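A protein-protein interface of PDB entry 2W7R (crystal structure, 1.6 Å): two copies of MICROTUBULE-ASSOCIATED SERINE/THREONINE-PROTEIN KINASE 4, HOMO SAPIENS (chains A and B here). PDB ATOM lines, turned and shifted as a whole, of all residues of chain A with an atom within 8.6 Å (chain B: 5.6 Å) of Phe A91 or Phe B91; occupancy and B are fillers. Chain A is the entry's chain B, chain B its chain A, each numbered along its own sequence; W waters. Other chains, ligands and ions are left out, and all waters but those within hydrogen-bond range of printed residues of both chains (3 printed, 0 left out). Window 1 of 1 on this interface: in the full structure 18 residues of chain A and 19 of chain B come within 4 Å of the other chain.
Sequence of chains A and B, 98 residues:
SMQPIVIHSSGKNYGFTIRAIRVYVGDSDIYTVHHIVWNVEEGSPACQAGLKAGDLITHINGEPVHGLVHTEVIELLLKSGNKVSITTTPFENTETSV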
ATOM      1  N   ARG A  19      -5.902   5.625  -0.129  1.00  0.00           N
ATOM      2  CA  ARG A  19      -6.116   6.364  -1.366  1.00  0.00           C
ATOM      3  C   ARG A  19      -6.029   7.845  -1.089  1.00  0.00           C
ATOM      4  O   ARG A  19      -6.346   8.301   0.011  1.00  0.00           O
ATOM      5  CB  ARG A  19      -7.490   6.068  -1.958  1.00  0.00           C
ATOM      6  CG  ARG A  19      -7.599   4.693  -2.592  1.00  0.00           C
ATOM      7  CD  ARG A  19      -8.988   4.493  -3.161  1.00  0.00           C
ATOM      8  NE  ARG A  19      -9.107   3.230  -3.901  1.00  0.00           N
ATOM      9  CZ  ARG A  19     -10.161   2.902  -4.646  1.00  0.00           C
ATOM     10  NH1 ARG A  19     -11.189   3.732  -4.745  1.00  0.00           N
ATOM     11  NH2 ARG A  19     -10.194   1.744  -5.291  1.00  0.00           N
ATOM     12  N   ALA A  20      -5.588   8.601  -2.087  1.00  0.00           N
ATOM     13  CA  ALA A  20      -5.612  10.045  -1.992  1.00  0.00           C
ATOM     14  C   ALA A  20      -6.911  10.537  -2.601  1.00  0.00           C
ATOM     15  O   ALA A  20      -7.333  10.047  -3.648  1.00  0.00           O
ATOM     16  CB  ALA A  20      -4.433  10.649  -2.747  1.00  0.00           C
ATOM     17  N   ILE A  21      -7.546  11.499  -1.950  1.00  0.00           N
ATOM     18  CA  ILE A  21      -8.753  12.077  -2.507  1.00  0.00           C
ATOM     19  C   ILE A  21      -8.603  13.572  -2.572  1.00  0.00           C
ATOM     20  O   ILE A  21      -7.861  14.161  -1.771  1.00  0.00           O
ATOM     21  CB  ILE A  21     -10.001  11.704  -1.678  1.00  0.00           C
ATOM     22  CG1 ILE A  21     -10.040  12.457  -0.344  1.00  0.00           C
ATOM     23  CG2 ILE A  21     -10.035  10.189  -1.446  1.00  0.00           C
ATOM     24  CD1 ILE A  21     -11.290  12.141   0.461  1.00  0.00           C
ATOM     25  N   ARG A  22      -9.286  14.183  -3.530  1.00  0.00           N
ATOM     26  CA  ARG A  22      -9.379  15.635  -3.609  1.00  0.00           C
ATOM     27  C   ARG A  22     -10.802  16.054  -3.304  1.00  0.00           C
ATOM     28  O   ARG A  22     -11.754  15.528  -3.890  1.00  0.00           O
ATOM     29  CB  ARG A  22      -9.002  16.165  -4.996  1.00  0.00           C
ATOM     30  CG  ARG A  22      -7.546  15.957  -5.385  1.00  0.00           C
ATOM     31  CD  ARG A  22      -7.296  16.581  -6.750  1.00  0.00           C
ATOM     32  NE  ARG A  22      -5.950  16.315  -7.243  1.00  0.00           N
ATOM     33  CZ  ARG A  22      -5.481  16.795  -8.392  1.00  0.00           C
ATOM     34  NH1 ARG A  22      -6.252  17.571  -9.150  1.00  0.00           N
ATOM     35  NH2 ARG A  22      -4.242  16.502  -8.783  1.00  0.00           N
ATOM     36  N   VAL A  23     -10.941  17.000  -2.387  1.00  0.00           N
ATOM     37  CA  VAL A  23     -12.245  17.540  -2.020  1.00  0.00           C
ATOM     38  C   VAL A  23     -12.327  18.985  -2.501  1.00  0.00           C
ATOM     39  O   VAL A  23     -11.582  19.854  -2.017  1.00  0.00           O
ATOM     40  CB  VAL A  23     -12.476  17.460  -0.502  1.00  0.00           C
ATOM     41  CG1 VAL A  23     -13.789  18.128  -0.119  1.00  0.00           C
ATOM     42  CG2 VAL A  23     -12.458  16.007  -0.021  1.00  0.00           C
ATOM     43  N   THR A  32      -8.756  20.484  -1.393  1.00  0.00           N
ATOM     44  CA  THR A  32      -7.819  20.007  -0.385  1.00  0.00           C
ATOM     45  C   THR A  32      -7.620  18.514  -0.581  1.00  0.00           C
ATOM     46  O   THR A  32      -8.474  17.834  -1.152  1.00  0.00           O
ATOM     47  CB  THR A  32      -8.286  20.294   1.057  1.00  0.00           C
ATOM     48  OG1 THR A  32      -9.621  19.816   1.253  1.00  0.00           O
ATOM     49  CG2 THR A  32      -8.229  21.804   1.356  1.00  0.00           C
ATOM     50  N   HIS A  34      -6.822  14.651   0.937  1.00  0.00           N
ATOM     51  CA  HIS A  34      -6.999  13.822   2.110  1.00  0.00           C
ATOM     52  C   HIS A  34      -6.591  12.399   1.814  1.00  0.00           C
ATOM     53  O   HIS A  34      -6.724  11.920   0.689  1.00  0.00           O
ATOM     54  CB  HIS A  34      -8.441  13.910   2.602  1.00  0.00           C
ATOM     55  CG  HIS A  34      -8.901  15.317   2.783  1.00  0.00           C
ATOM     56  ND1 HIS A  34      -8.820  15.973   3.991  1.00  0.00           N
ATOM     57  CD2 HIS A  34      -9.369  16.220   1.891  1.00  0.00           C
ATOM     58  CE1 HIS A  34      -9.255  17.212   3.843  1.00  0.00           C
ATOM     59  NE2 HIS A  34      -9.595  17.388   2.579  1.00  0.00           N
ATOM     60  N   HIS A  35      -6.035  11.741   2.818  1.00  0.00           N
ATOM     61  CA  HIS A  35      -5.541  10.393   2.650  1.00  0.00           C
ATOM     62  C   HIS A  35      -6.436   9.463   3.432  1.00  0.00           C
ATOM     63  O   HIS A  35      -6.397   9.429   4.665  1.00  0.00           O
ATOM     64  CB  HIS A  35      -4.083  10.309   3.081  1.00  0.00           C
ATOM     65  CG  HIS A  35      -3.209  11.292   2.363  1.00  0.00           C
ATOM     66  ND1 HIS A  35      -2.643  11.015   1.137  1.00  0.00           N
ATOM     67  CD2 HIS A  35      -2.857  12.564   2.663  1.00  0.00           C
ATOM     68  CE1 HIS A  35      -1.967  12.071   0.717  1.00  0.00           C
ATOM     69  NE2 HIS A  35      -2.074  13.022   1.629  1.00  0.00           N
ATOM     70  N   ILE A  36      -7.258   8.726   2.696  1.00  0.00           N
ATOM     71  CA  ILE A  36      -8.280   7.892   3.307  1.00  0.00           C
ATOM     72  C   ILE A  36      -7.821   6.447   3.495  1.00  0.00           C
ATOM     73  O   ILE A  36      -7.144   5.880   2.639  1.00  0.00           O
ATOM     74  CB  ILE A  36      -9.588   7.928   2.476  1.00  0.00           C
ATOM     75  CG1 ILE A  36     -10.721   7.208   3.213  1.00  0.00           C
ATOM     76  CG2 ILE A  36      -9.368   7.324   1.075  1.00  0.00           C
ATOM     77  CD1 ILE A  36     -12.107   7.597   2.722  1.00  0.00           C
ATOM     78  N   VAL A  37      -8.158   5.865   4.643  1.00  0.00           N
ATOM     79  CA  VAL A  37      -7.979   4.425   4.808  1.00  0.00           C
ATOM     80  C   VAL A  37      -9.075   3.770   3.983  1.00  0.00           C
ATOM     81  O   VAL A  37     -10.244   3.788   4.374  1.00  0.00           O
ATOM     82  CB  VAL A  37      -8.115   3.997   6.274  1.00  0.00           C
ATOM     83  CG1 VAL A  37      -7.901   2.485   6.419  1.00  0.00           C
ATOM     84  CG2 VAL A  37      -7.140   4.769   7.129  1.00  0.00           C
ATOM     85  N   TRP A  38      -8.701   3.230   2.828  1.00  0.00           N
ATOM     86  CA  TRP A  38      -9.670   2.675   1.892  1.00  0.00           C
ATOM     87  C   TRP A  38     -10.152   1.292   2.331  1.00  0.00           C
ATOM     88  O   TRP A  38     -11.335   0.977   2.246  1.00  0.00           O
ATOM     89  CB  TRP A  38      -9.071   2.593   0.488  1.00  0.00           C
ATOM     90  CG  TRP A  38     -10.053   2.141  -0.501  1.00  0.00           C
ATOM     91  CD1 TRP A  38      -9.990   1.005  -1.250  1.00  0.00           C
ATOM     92  CD2 TRP A  38     -11.282   2.788  -0.848  1.00  0.00           C
ATOM     93  NE1 TRP A  38     -11.099   0.907  -2.053  1.00  0.00           N
ATOM     94  CE2 TRP A  38     -11.910   1.986  -1.827  1.00  0.00           C
ATOM     95  CE3 TRP A  38     -11.917   3.961  -0.427  1.00  0.00           C
ATOM     96  CZ2 TRP A  38     -13.141   2.323  -2.391  1.00  0.00           C
ATOM     97  CZ3 TRP A  38     -13.136   4.298  -0.996  1.00  0.00           C
ATOM     98  CH2 TRP A  38     -13.731   3.484  -1.970  1.00  0.00           C
ATOM     99  N   ASN A  39      -9.222   0.470   2.795  1.00  0.00           N
ATOM    100  CA  ASN A  39      -9.552  -0.887   3.194  1.00  0.00           C
ATOM    101  C   ASN A  39      -8.679  -1.351   4.333  1.00  0.00           C
ATOM    102  O   ASN A  39      -7.507  -0.983   4.407  1.00  0.00           O
ATOM    103  CB  ASN A  39      -9.377  -1.861   2.025  1.00  0.00           C
ATOM    104  CG  ASN A  39      -9.821  -3.264   2.379  1.00  0.00           C
ATOM    105  OD1 ASN A  39     -11.013  -3.519   2.542  1.00  0.00           O
ATOM    106  ND2 ASN A  39      -8.865  -4.186   2.504  1.00  0.00           N
ATOM    107  N   LYS A  52      -9.746   2.060  11.193  1.00  0.00           N
ATOM    108  CA  LYS A  52     -11.094   2.011  10.635  1.00  0.00           C
ATOM    109  C   LYS A  52     -11.142   2.490   9.194  1.00  0.00           C
ATOM    110  O   LYS A  52     -10.804   3.632   8.907  1.00  0.00           O
ATOM    111  CB  LYS A  52     -12.039   2.860  11.484  1.00  0.00           C
ATOM    112  CG  LYS A  52     -13.514   2.649  11.190  1.00  0.00           C
ATOM    113  CD  LYS A  52     -14.376   3.367  12.220  1.00  0.00           C
ATOM    114  CE  LYS A  52     -15.853   3.080  12.007  1.00  0.00           C
ATOM    115  NZ  LYS A  52     -16.317   3.502  10.656  1.00  0.00           N
ATOM    116  N   ALA A  53     -11.586   1.620   8.289  1.00  0.00           N
ATOM    117  CA  ALA A  53     -11.784   2.032   6.910  1.00  0.00           C
ATOM    118  C   ALA A  53     -12.785   3.178   6.855  1.00  0.00           C
ATOM    119  O   ALA A  53     -13.778   3.184   7.591  1.00  0.00           O
ATOM    120  CB  ALA A  53     -12.260   0.848   6.061  1.00  0.00           C
ATOM    121  N   GLY A  54     -12.504   4.165   6.009  1.00  0.00           N
ATOM    122  CA  GLY A  54     -13.359   5.333   5.878  1.00  0.00           C
ATOM    123  C   GLY A  54     -12.836   6.559   6.602  1.00  0.00           C
ATOM    124  O   GLY A  54     -13.257   7.669   6.305  1.00  0.00           O
ATOM    125  N   ASP A  55     -11.940   6.352   7.564  1.00  0.00           N
ATOM    126  CA  ASP A  55     -11.324   7.460   8.284  1.00  0.00           C
ATOM    127  C   ASP A  55     -10.151   8.046   7.507  1.00  0.00           C
ATOM    128  O   ASP A  55      -9.637   7.435   6.572  1.00  0.00           O
ATOM    129  CB  ASP A  55     -10.855   7.004   9.666  1.00  0.00           C
ATOM    130  CG  ASP A  55     -12.003   6.810  10.640  1.00  0.00           C
ATOM    131  OD1 ASP A  55     -13.154   7.153  10.291  1.00  0.00           O
ATOM    132  OD2 ASP A  55     -11.752   6.316  11.756  1.00  0.00           O
ATOM    133  N   LEU A  56      -9.717   9.231   7.913  1.00  0.00           N
ATOM    134  CA  LEU A  56      -8.644   9.929   7.234  1.00  0.00           C
ATOM    135  C   LEU A  56      -7.399   9.930   8.101  1.00  0.00           C
ATOM    136  O   LEU A  56      -7.476  10.091   9.324  1.00  0.00           O
ATOM    137  CB  LEU A  56      -9.057  11.373   6.912  1.00  0.00           C
ATOM    138  CG  LEU A  56     -10.347  11.555   6.099  1.00  0.00           C
ATOM    139  CD1 LEU A  56     -10.766  13.012   6.015  1.00  0.00           C
ATOM    140  CD2 LEU A  56     -10.158  10.939   4.703  1.00  0.00           C
ATOM    141  N   THR A  88      -5.771   9.183  13.165  1.00  0.00           N
ATOM    142  CA  THR A  88      -6.874   9.274  12.214  1.00  0.00           C
ATOM    143  C   THR A  88      -8.004  10.157  12.739  1.00  0.00           C
ATOM    144  O   THR A  88      -8.086  10.440  13.939  1.00  0.00           O
ATOM    145  CB  THR A  88      -7.455   7.885  11.852  1.00  0.00           C
ATOM    146  OG1 THR A  88      -8.007   7.282  13.026  1.00  0.00           O
ATOM    147  CG2 THR A  88      -6.376   6.976  11.268  1.00  0.00           C
ATOM    148  N   THR A  89      -8.850  10.604  11.819  1.00  0.00           N
ATOM    149  CA  THR A  89     -10.053  11.353  12.147  1.00  0.00           C
ATOM    150  C   THR A  89     -11.169  10.920  11.204  1.00  0.00           C
ATOM    151  O   THR A  89     -10.914  10.589  10.045  1.00  0.00           O
ATOM    152  CB  THR A  89      -9.822  12.876  11.985  1.00  0.00           C
ATOM    153  OG1 THR A  89     -10.928  13.595  12.543  1.00  0.00           O
ATOM    154  CG2 THR A  89      -9.672  13.248  10.517  1.00  0.00           C
ATOM    155  N   PRO A  90     -12.414  10.916  11.690  1.00  0.00           N
ATOM    156  CA  PRO A  90     -13.556  10.642  10.816  1.00  0.00           C
ATOM    157  C   PRO A  90     -13.924  11.907  10.049  1.00  0.00           C
ATOM    158  O   PRO A  90     -13.435  12.983  10.393  1.00  0.00           O
ATOM    159  CB  PRO A  90     -14.680  10.293  11.804  1.00  0.00           C
ATOM    160  CG  PRO A  90     -14.035  10.273  13.187  1.00  0.00           C
ATOM    161  CD  PRO A  90     -12.837  11.151  13.080  1.00  0.00           C
ATOM    162  N   PHE A  91     -14.744  11.787   9.009  1.00  0.00           N
ATOM    163  CA  PHE A  91     -15.331  12.976   8.410  1.00  0.00           C
ATOM    164  C   PHE A  91     -16.199  13.654   9.466  1.00  0.00           C
ATOM    165  O   PHE A  91     -17.218  13.113   9.893  1.00  0.00           O
ATOM    166  CB  PHE A  91     -16.165  12.637   7.168  1.00  0.00           C
ATOM    167  CG  PHE A  91     -15.345  12.336   5.943  1.00  0.00           C
ATOM    168  CD1 PHE A  91     -15.045  11.026   5.597  1.00  0.00           C
ATOM    169  CD2 PHE A  91     -14.890  13.361   5.124  1.00  0.00           C
ATOM    170  CE1 PHE A  91     -14.296  10.748   4.469  1.00  0.00           C
ATOM    171  CE2 PHE A  91     -14.137  13.090   3.999  1.00  0.00           C
ATOM    172  CZ  PHE A  91     -13.846  11.782   3.663  1.00  0.00           C
ATOM    173  N   GLU A  92     -15.764  14.827   9.903  1.00  0.00           N
ATOM    174  CA  GLU A  92     -16.487  15.623  10.888  1.00  0.00           C
ATOM    175  C   GLU A  92     -16.220  17.076  10.552  1.00  0.00           C
ATOM    176  O   GLU A  92     -15.160  17.611  10.882  1.00  0.00           O
ATOM    177  CB  GLU A  92     -15.993  15.337  12.307  1.00  0.00           C
ATOM    178  CG  GLU A  92     -16.417  13.999  12.890  1.00  0.00           C
ATOM    179  CD  GLU A  92     -16.225  13.943  14.400  1.00  0.00           C
ATOM    180  OE1 GLU A  92     -16.474  14.970  15.070  1.00  0.00           O
ATOM    181  OE2 GLU A  92     -15.832  12.875  14.918  1.00  0.00           O
ATOM    182  N   ASN A  93     -17.173  17.709   9.880  1.00  0.00           N
ATOM    183  CA  ASN A  93     -16.961  19.064   9.384  1.00  0.00           C
ATOM    184  C   ASN A  93     -17.934  20.057  10.025  1.00  0.00           C
ATOM    185  O   ASN A  93     -18.355  21.033   9.399  1.00  0.00           O
ATOM    186  CB  ASN A  93     -17.052  19.074   7.855  1.00  0.00           C
ATOM    187  CG  ASN A  93     -15.979  18.202   7.200  1.00  0.00           C
ATOM    188  OD1 ASN A  93     -14.785  18.403   7.421  1.00  0.00           O
ATOM    189  ND2 ASN A  93     -16.404  17.233   6.393  1.00  0.00           N
ATOM    190  N   THR A  94     -18.266  19.797  11.289  1.00  0.00           N
ATOM    191  CA  THR A  94     -19.220  20.605  12.051  1.00  0.00           C
ATOM    192  C   THR A  94     -18.718  22.023  12.340  1.00  0.00           C
ATOM    193  O   THR A  94     -17.618  22.202  12.863  1.00  0.00           O
ATOM    194  CB  THR A  94     -19.543  19.931  13.402  1.00  0.00           C
ATOM    195  OG1 THR A  94     -20.001  18.590  13.173  1.00  0.00           O
ATOM    196  CG2 THR A  94     -20.611  20.714  14.157  1.00  0.00           C
ATOM    197  N   ILE B  21     -15.969  15.416  -5.169  1.00  0.00           N
ATOM    198  CA  ILE B  21     -14.661  14.853  -4.840  1.00  0.00           C
ATOM    199  C   ILE B  21     -14.101  14.047  -5.985  1.00  0.00           C
ATOM    200  O   ILE B  21     -14.846  13.595  -6.872  1.00  0.00           O
ATOM    201  CB  ILE B  21     -14.702  13.961  -3.568  1.00  0.00           C
ATOM    202  CG1 ILE B  21     -15.461  12.651  -3.814  1.00  0.00           C
ATOM    203  CG2 ILE B  21     -15.303  14.743  -2.395  1.00  0.00           C
ATOM    204  CD1 ILE B  21     -15.381  11.705  -2.625  1.00  0.00           C
ATOM    205  N   VAL B  23     -11.557  10.590  -6.360  1.00  0.00           N
ATOM    206  CA  VAL B  23     -10.914   9.536  -5.588  1.00  0.00           C
ATOM    207  C   VAL B  23      -9.898   8.829  -6.471  1.00  0.00           C
ATOM    208  O   VAL B  23     -10.260   8.216  -7.484  1.00  0.00           O
ATOM    209  CB  VAL B  23     -11.952   8.548  -5.059  1.00  0.00           C
ATOM    210  CG1 VAL B  23     -11.264   7.410  -4.311  1.00  0.00           C
ATOM    211  CG2 VAL B  23     -12.939   9.275  -4.152  1.00  0.00           C
ATOM    212  N   ILE B  36     -20.143  14.079  -2.034  1.00  0.00           N
ATOM    213  CA  ILE B  36     -20.106  13.662  -0.651  1.00  0.00           C
ATOM    214  C   ILE B  36     -20.879  14.647   0.210  1.00  0.00           C
ATOM    215  O   ILE B  36     -20.907  15.844  -0.074  1.00  0.00           O
ATOM    216  CB  ILE B  36     -18.637  13.564  -0.169  1.00  0.00           C
ATOM    217  CG1 ILE B  36     -18.530  12.785   1.129  1.00  0.00           C
ATOM    218  CG2 ILE B  36     -18.009  14.944  -0.035  1.00  0.00           C
ATOM    219  CD1 ILE B  36     -17.091  12.592   1.585  1.00  0.00           C
ATOM    220  N   TRP B  38     -20.724  16.849   3.022  1.00  0.00           N
ATOM    221  CA  TRP B  38     -19.546  17.422   3.671  1.00  0.00           C
ATOM    222  C   TRP B  38     -19.803  17.780   5.126  1.00  0.00           C
ATOM    223  O   TRP B  38     -18.990  17.501   6.005  1.00  0.00           O
ATOM    224  CB  TRP B  38     -19.030  18.648   2.905  1.00  0.00           C
ATOM    225  CG  TRP B  38     -17.717  19.119   3.439  1.00  0.00           C
ATOM    226  CD1 TRP B  38     -17.461  20.304   4.080  1.00  0.00           C
ATOM    227  CD2 TRP B  38     -16.478  18.397   3.426  1.00  0.00           C
ATOM    228  NE1 TRP B  38     -16.138  20.364   4.453  1.00  0.00           N
ATOM    229  CE2 TRP B  38     -15.513  19.209   4.063  1.00  0.00           C
ATOM    230  CE3 TRP B  38     -16.088  17.149   2.929  1.00  0.00           C
ATOM    231  CZ2 TRP B  38     -14.185  18.814   4.213  1.00  0.00           C
ATOM    232  CZ3 TRP B  38     -14.772  16.754   3.090  1.00  0.00           C
ATOM    233  CH2 TRP B  38     -13.836  17.586   3.723  1.00  0.00           C
ATOM    234  N   ALA B  53     -21.988  13.190   7.545  1.00  0.00           N
ATOM    235  CA  ALA B  53     -20.800  13.651   6.842  1.00  0.00           C
ATOM    236  C   ALA B  53     -19.953  12.458   6.421  1.00  0.00           C
ATOM    237  O   ALA B  53     -19.767  11.513   7.195  1.00  0.00           O
ATOM    238  CB  ALA B  53     -19.996  14.588   7.720  1.00  0.00           C
ATOM    239  N   GLY B  54     -19.452  12.505   5.192  1.00  0.00           N
ATOM    240  CA  GLY B  54     -18.699  11.397   4.638  1.00  0.00           C
ATOM    241  C   GLY B  54     -19.506  10.447   3.768  1.00  0.00           C
ATOM    242  O   GLY B  54     -18.931   9.673   3.017  1.00  0.00           O
ATOM    243  N   ASP B  55     -20.831  10.497   3.881  1.00  0.00           N
ATOM    244  CA  ASP B  55     -21.709   9.683   3.051  1.00  0.00           C
ATOM    245  C   ASP B  55     -21.596  10.111   1.596  1.00  0.00           C
ATOM    246  O   ASP B  55     -21.657  11.303   1.290  1.00  0.00           O
ATOM    247  CB  ASP B  55     -23.163   9.851   3.505  1.00  0.00           C
ATOM    248  CG  ASP B  55     -23.478   9.076   4.770  1.00  0.00           C
ATOM    249  OD1 ASP B  55     -22.942   7.959   4.937  1.00  0.00           O
ATOM    250  OD2 ASP B  55     -24.274   9.581   5.586  1.00  0.00           O
ATOM    251  N   LEU B  56     -21.435   9.146   0.693  1.00  0.00           N
ATOM    252  CA  LEU B  56     -21.500   9.446  -0.728  1.00  0.00           C
ATOM    253  C   LEU B  56     -22.949   9.379  -1.169  1.00  0.00           C
ATOM    254  O   LEU B  56     -23.663   8.435  -0.829  1.00  0.00           O
ATOM    255  CB  LEU B  56     -20.679   8.445  -1.555  1.00  0.00           C
ATOM    256  CG  LEU B  56     -19.170   8.366  -1.331  1.00  0.00           C
ATOM    257  CD1 LEU B  56     -18.545   7.394  -2.299  1.00  0.00           C
ATOM    258  CD2 LEU B  56     -18.529   9.739  -1.485  1.00  0.00           C
ATOM    259  N   THR B  89     -24.279   5.721   0.058  1.00  0.00           N
ATOM    260  CA  THR B  89     -23.501   4.497   0.137  1.00  0.00           C
ATOM    261  C   THR B  89     -22.217   4.764   0.930  1.00  0.00           C
ATOM    262  O   THR B  89     -21.733   5.892   0.965  1.00  0.00           O
ATOM    263  CB  THR B  89     -23.164   3.985  -1.276  1.00  0.00           C
ATOM    264  OG1 THR B  89     -22.669   2.643  -1.204  1.00  0.00           O
ATOM    265  CG2 THR B  89     -22.125   4.883  -1.943  1.00  0.00           C
ATOM    266  N   PRO B  90     -21.669   3.727   1.582  1.00  0.00           N
ATOM    267  CA  PRO B  90     -20.460   3.910   2.397  1.00  0.00           C
ATOM    268  C   PRO B  90     -19.263   4.385   1.574  1.00  0.00           C
ATOM    269  O   PRO B  90     -19.087   3.948   0.436  1.00  0.00           O
ATOM    270  CB  PRO B  90     -20.187   2.503   2.942  1.00  0.00           C
ATOM    271  CG  PRO B  90     -21.505   1.800   2.877  1.00  0.00           C
ATOM    272  CD  PRO B  90     -22.211   2.362   1.685  1.00  0.00           C
ATOM    273  N   PHE B  91     -18.454   5.270   2.152  1.00  0.00           N
ATOM    274  CA  PHE B  91     -17.245   5.759   1.494  1.00  0.00           C
ATOM    275  C   PHE B  91     -16.044   4.950   2.002  1.00  0.00           C
ATOM    276  O   PHE B  91     -15.290   5.385   2.876  1.00  0.00           O
ATOM    277  CB  PHE B  91     -17.088   7.272   1.736  1.00  0.00           C
ATOM    278  CG  PHE B  91     -15.989   7.925   0.937  1.00  0.00           C
ATOM    279  CD1 PHE B  91     -15.335   7.252  -0.082  1.00  0.00           C
ATOM    280  CD2 PHE B  91     -15.625   9.228   1.208  1.00  0.00           C
ATOM    281  CE1 PHE B  91     -14.324   7.877  -0.810  1.00  0.00           C
ATOM    282  CE2 PHE B  91     -14.627   9.861   0.483  1.00  0.00           C
ATOM    283  CZ  PHE B  91     -13.969   9.185  -0.521  1.00  0.00           C
ATOM    284  N   GLU B  92     -15.901   3.752   1.456  1.00  0.00           N
ATOM    285  CA  GLU B  92     -14.846   2.824   1.838  1.00  0.00           C
ATOM    286  C   GLU B  92     -14.939   1.647   0.892  1.00  0.00           C
ATOM    287  O   GLU B  92     -15.911   1.525   0.153  1.00  0.00           O
ATOM    288  CB  GLU B  92     -15.030   2.335   3.274  1.00  0.00           C
ATOM    289  CG  GLU B  92     -16.394   1.724   3.573  1.00  0.00           C
ATOM    290  CD  GLU B  92     -16.543   1.295   5.029  1.00  0.00           C
ATOM    291  OE1 GLU B  92     -15.841   0.351   5.455  1.00  0.00           O
ATOM    292  OE2 GLU B  92     -17.368   1.901   5.745  1.00  0.00           O
ATOM    293  N   ASN B  93     -13.938   0.776   0.913  1.00  0.00           N
ATOM    294  CA  ASN B  93     -14.014  -0.416   0.079  1.00  0.00           C
ATOM    295  C   ASN B  93     -15.206  -1.275   0.495  1.00  0.00           C
ATOM    296  O   ASN B  93     -15.365  -1.589   1.674  1.00  0.00           O
ATOM    297  CB  ASN B  93     -12.737  -1.243   0.177  1.00  0.00           C
ATOM    298  CG  ASN B  93     -12.844  -2.543  -0.590  1.00  0.00           C
ATOM    299  OD1 ASN B  93     -13.283  -2.555  -1.743  1.00  0.00           O
ATOM    300  ND2 ASN B  93     -12.458  -3.646   0.047  1.00  0.00           N
HETATM  301  O   HOH W   1     -15.515   1.193   8.434  1.00  0.00           O
HETATM  302  O   HOH W   2     -11.556   5.506  -7.681  1.00  0.00           O
HETATM  303  O   HOH W   3     -18.727  10.814   9.602  1.00  0.00           O
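Hydrophobic or aromatic side chains of chain B that line the printed part of chain A: Ile B21, Val B23, Ile B36, Trp B38, Ala B53 and Phe B91. Hydrophobic or aromatic side chains of chain A within 4 Å of the printed part of chain B: Val A23, Ile A36, Trp A38, Ala A53 and Phe A91. Among the printed residues, 17 pairs touch across the chains. Among the printed residues, no Asp or Glu carboxylate lies within 4 Å of a Lys or Arg side-chain nitrogen of the other chain.
N of Val A23 lies within hydrogen-bond range of O of Thr A32 (2.9 Å). O of Arg A19 sits at hydrogen-bond distance from N of Ile A36, at 2.9 Å. O of Val A37 sits at hydrogen-bond distance from N of Gly A54 (2.8 Å).
Arg A19 touches Val B23 (NH1 to CG1, 3.7 Å). Ile B21 touches Arg A22. CG2 of Ile B21 touches CG2 of Val A23 (3.9 Å). CZ3 of Trp B38 touches CG1 of Val A23 (3.6 Å). Ile A36 touches Phe B91 (CD1 to O, 3.9 Å). Phe A91 touches Ile B36. Phe A91 touches Trp B38 (CE2 to CZ3, 3.8 Å). Ala B53 touches Phe A91. Gly B54 touches Phe A91 (CA to CG, 3.7 Å). Phe A91 touches Phe B91.
Of chain B, only Ile B36, Trp B38, Ala B53, Gly B54 and Phe B91 come within 4 Å of Phe A91. Of chain A, only Ile A36 (3.9 Å), Trp A38 (3.8 Å), Gly A54 (3.6 Å) and Phe A91 (3.8 Å) come within 4 Å of Phe B91. Of the printed residues of chain B, Asn A93 touches Trp B38 (2.6 Å). Printed residues of chain B within 4 Å of Arg A22: Ile B21 (3.1 Å). Of the printed residues of chain B, Gly A54 touches Phe B91. Leu A56 touches none of the printed residues of chain B. The nearest residue of chain A that does not touch Phe B91 is Ile A21 (4.04 Å).
Val A23 touches Trp B38, but with the chains exchanged Trp A38 does not touch Val B23 (4.9 Å). Trp A38 touches Glu B92, but with the chains exchanged Glu A92 does not touch Trp B38 (5.3 Å). Phe A91 touches Ala B53, but with the chains exchanged Ala A53 does not touch Phe B91 (5.2 Å). Phe B91 touches its own counterpart, Phe A91.
N of Asn B93 is in hydrogen-bond range of O of Trp A38 (2.9 Å). The side-chain amide oxygen (OD1) of Asn A39 lies within hydrogen-bond range of the side-chain amide nitrogen (ND2) of Asn B93, at 2.9 Å. The side-chain amide nitrogen (ND2) of Asn A93 sits at hydrogen-bond distance from the backbone carbonyl oxygen (O) of Trp B38, at 2.6 Å.
Water W3 lies within hydrogen-bond range of the backbone carbonyl oxygen of Ala B53 (2.7 Å) and the backbone carbonyl oxygen of Phe A91 (2.8 Å). Water W1 lies within hydrogen-bond range of O of Ala A53 (2.8 Å), OE1 of Glu B92 (3.1 Å) and NZ of Lys A52 (3.3 Å). Water W2 bridges O of Val B23 (3.0 Å) and NH1 of Arg A19 (3.4 Å).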
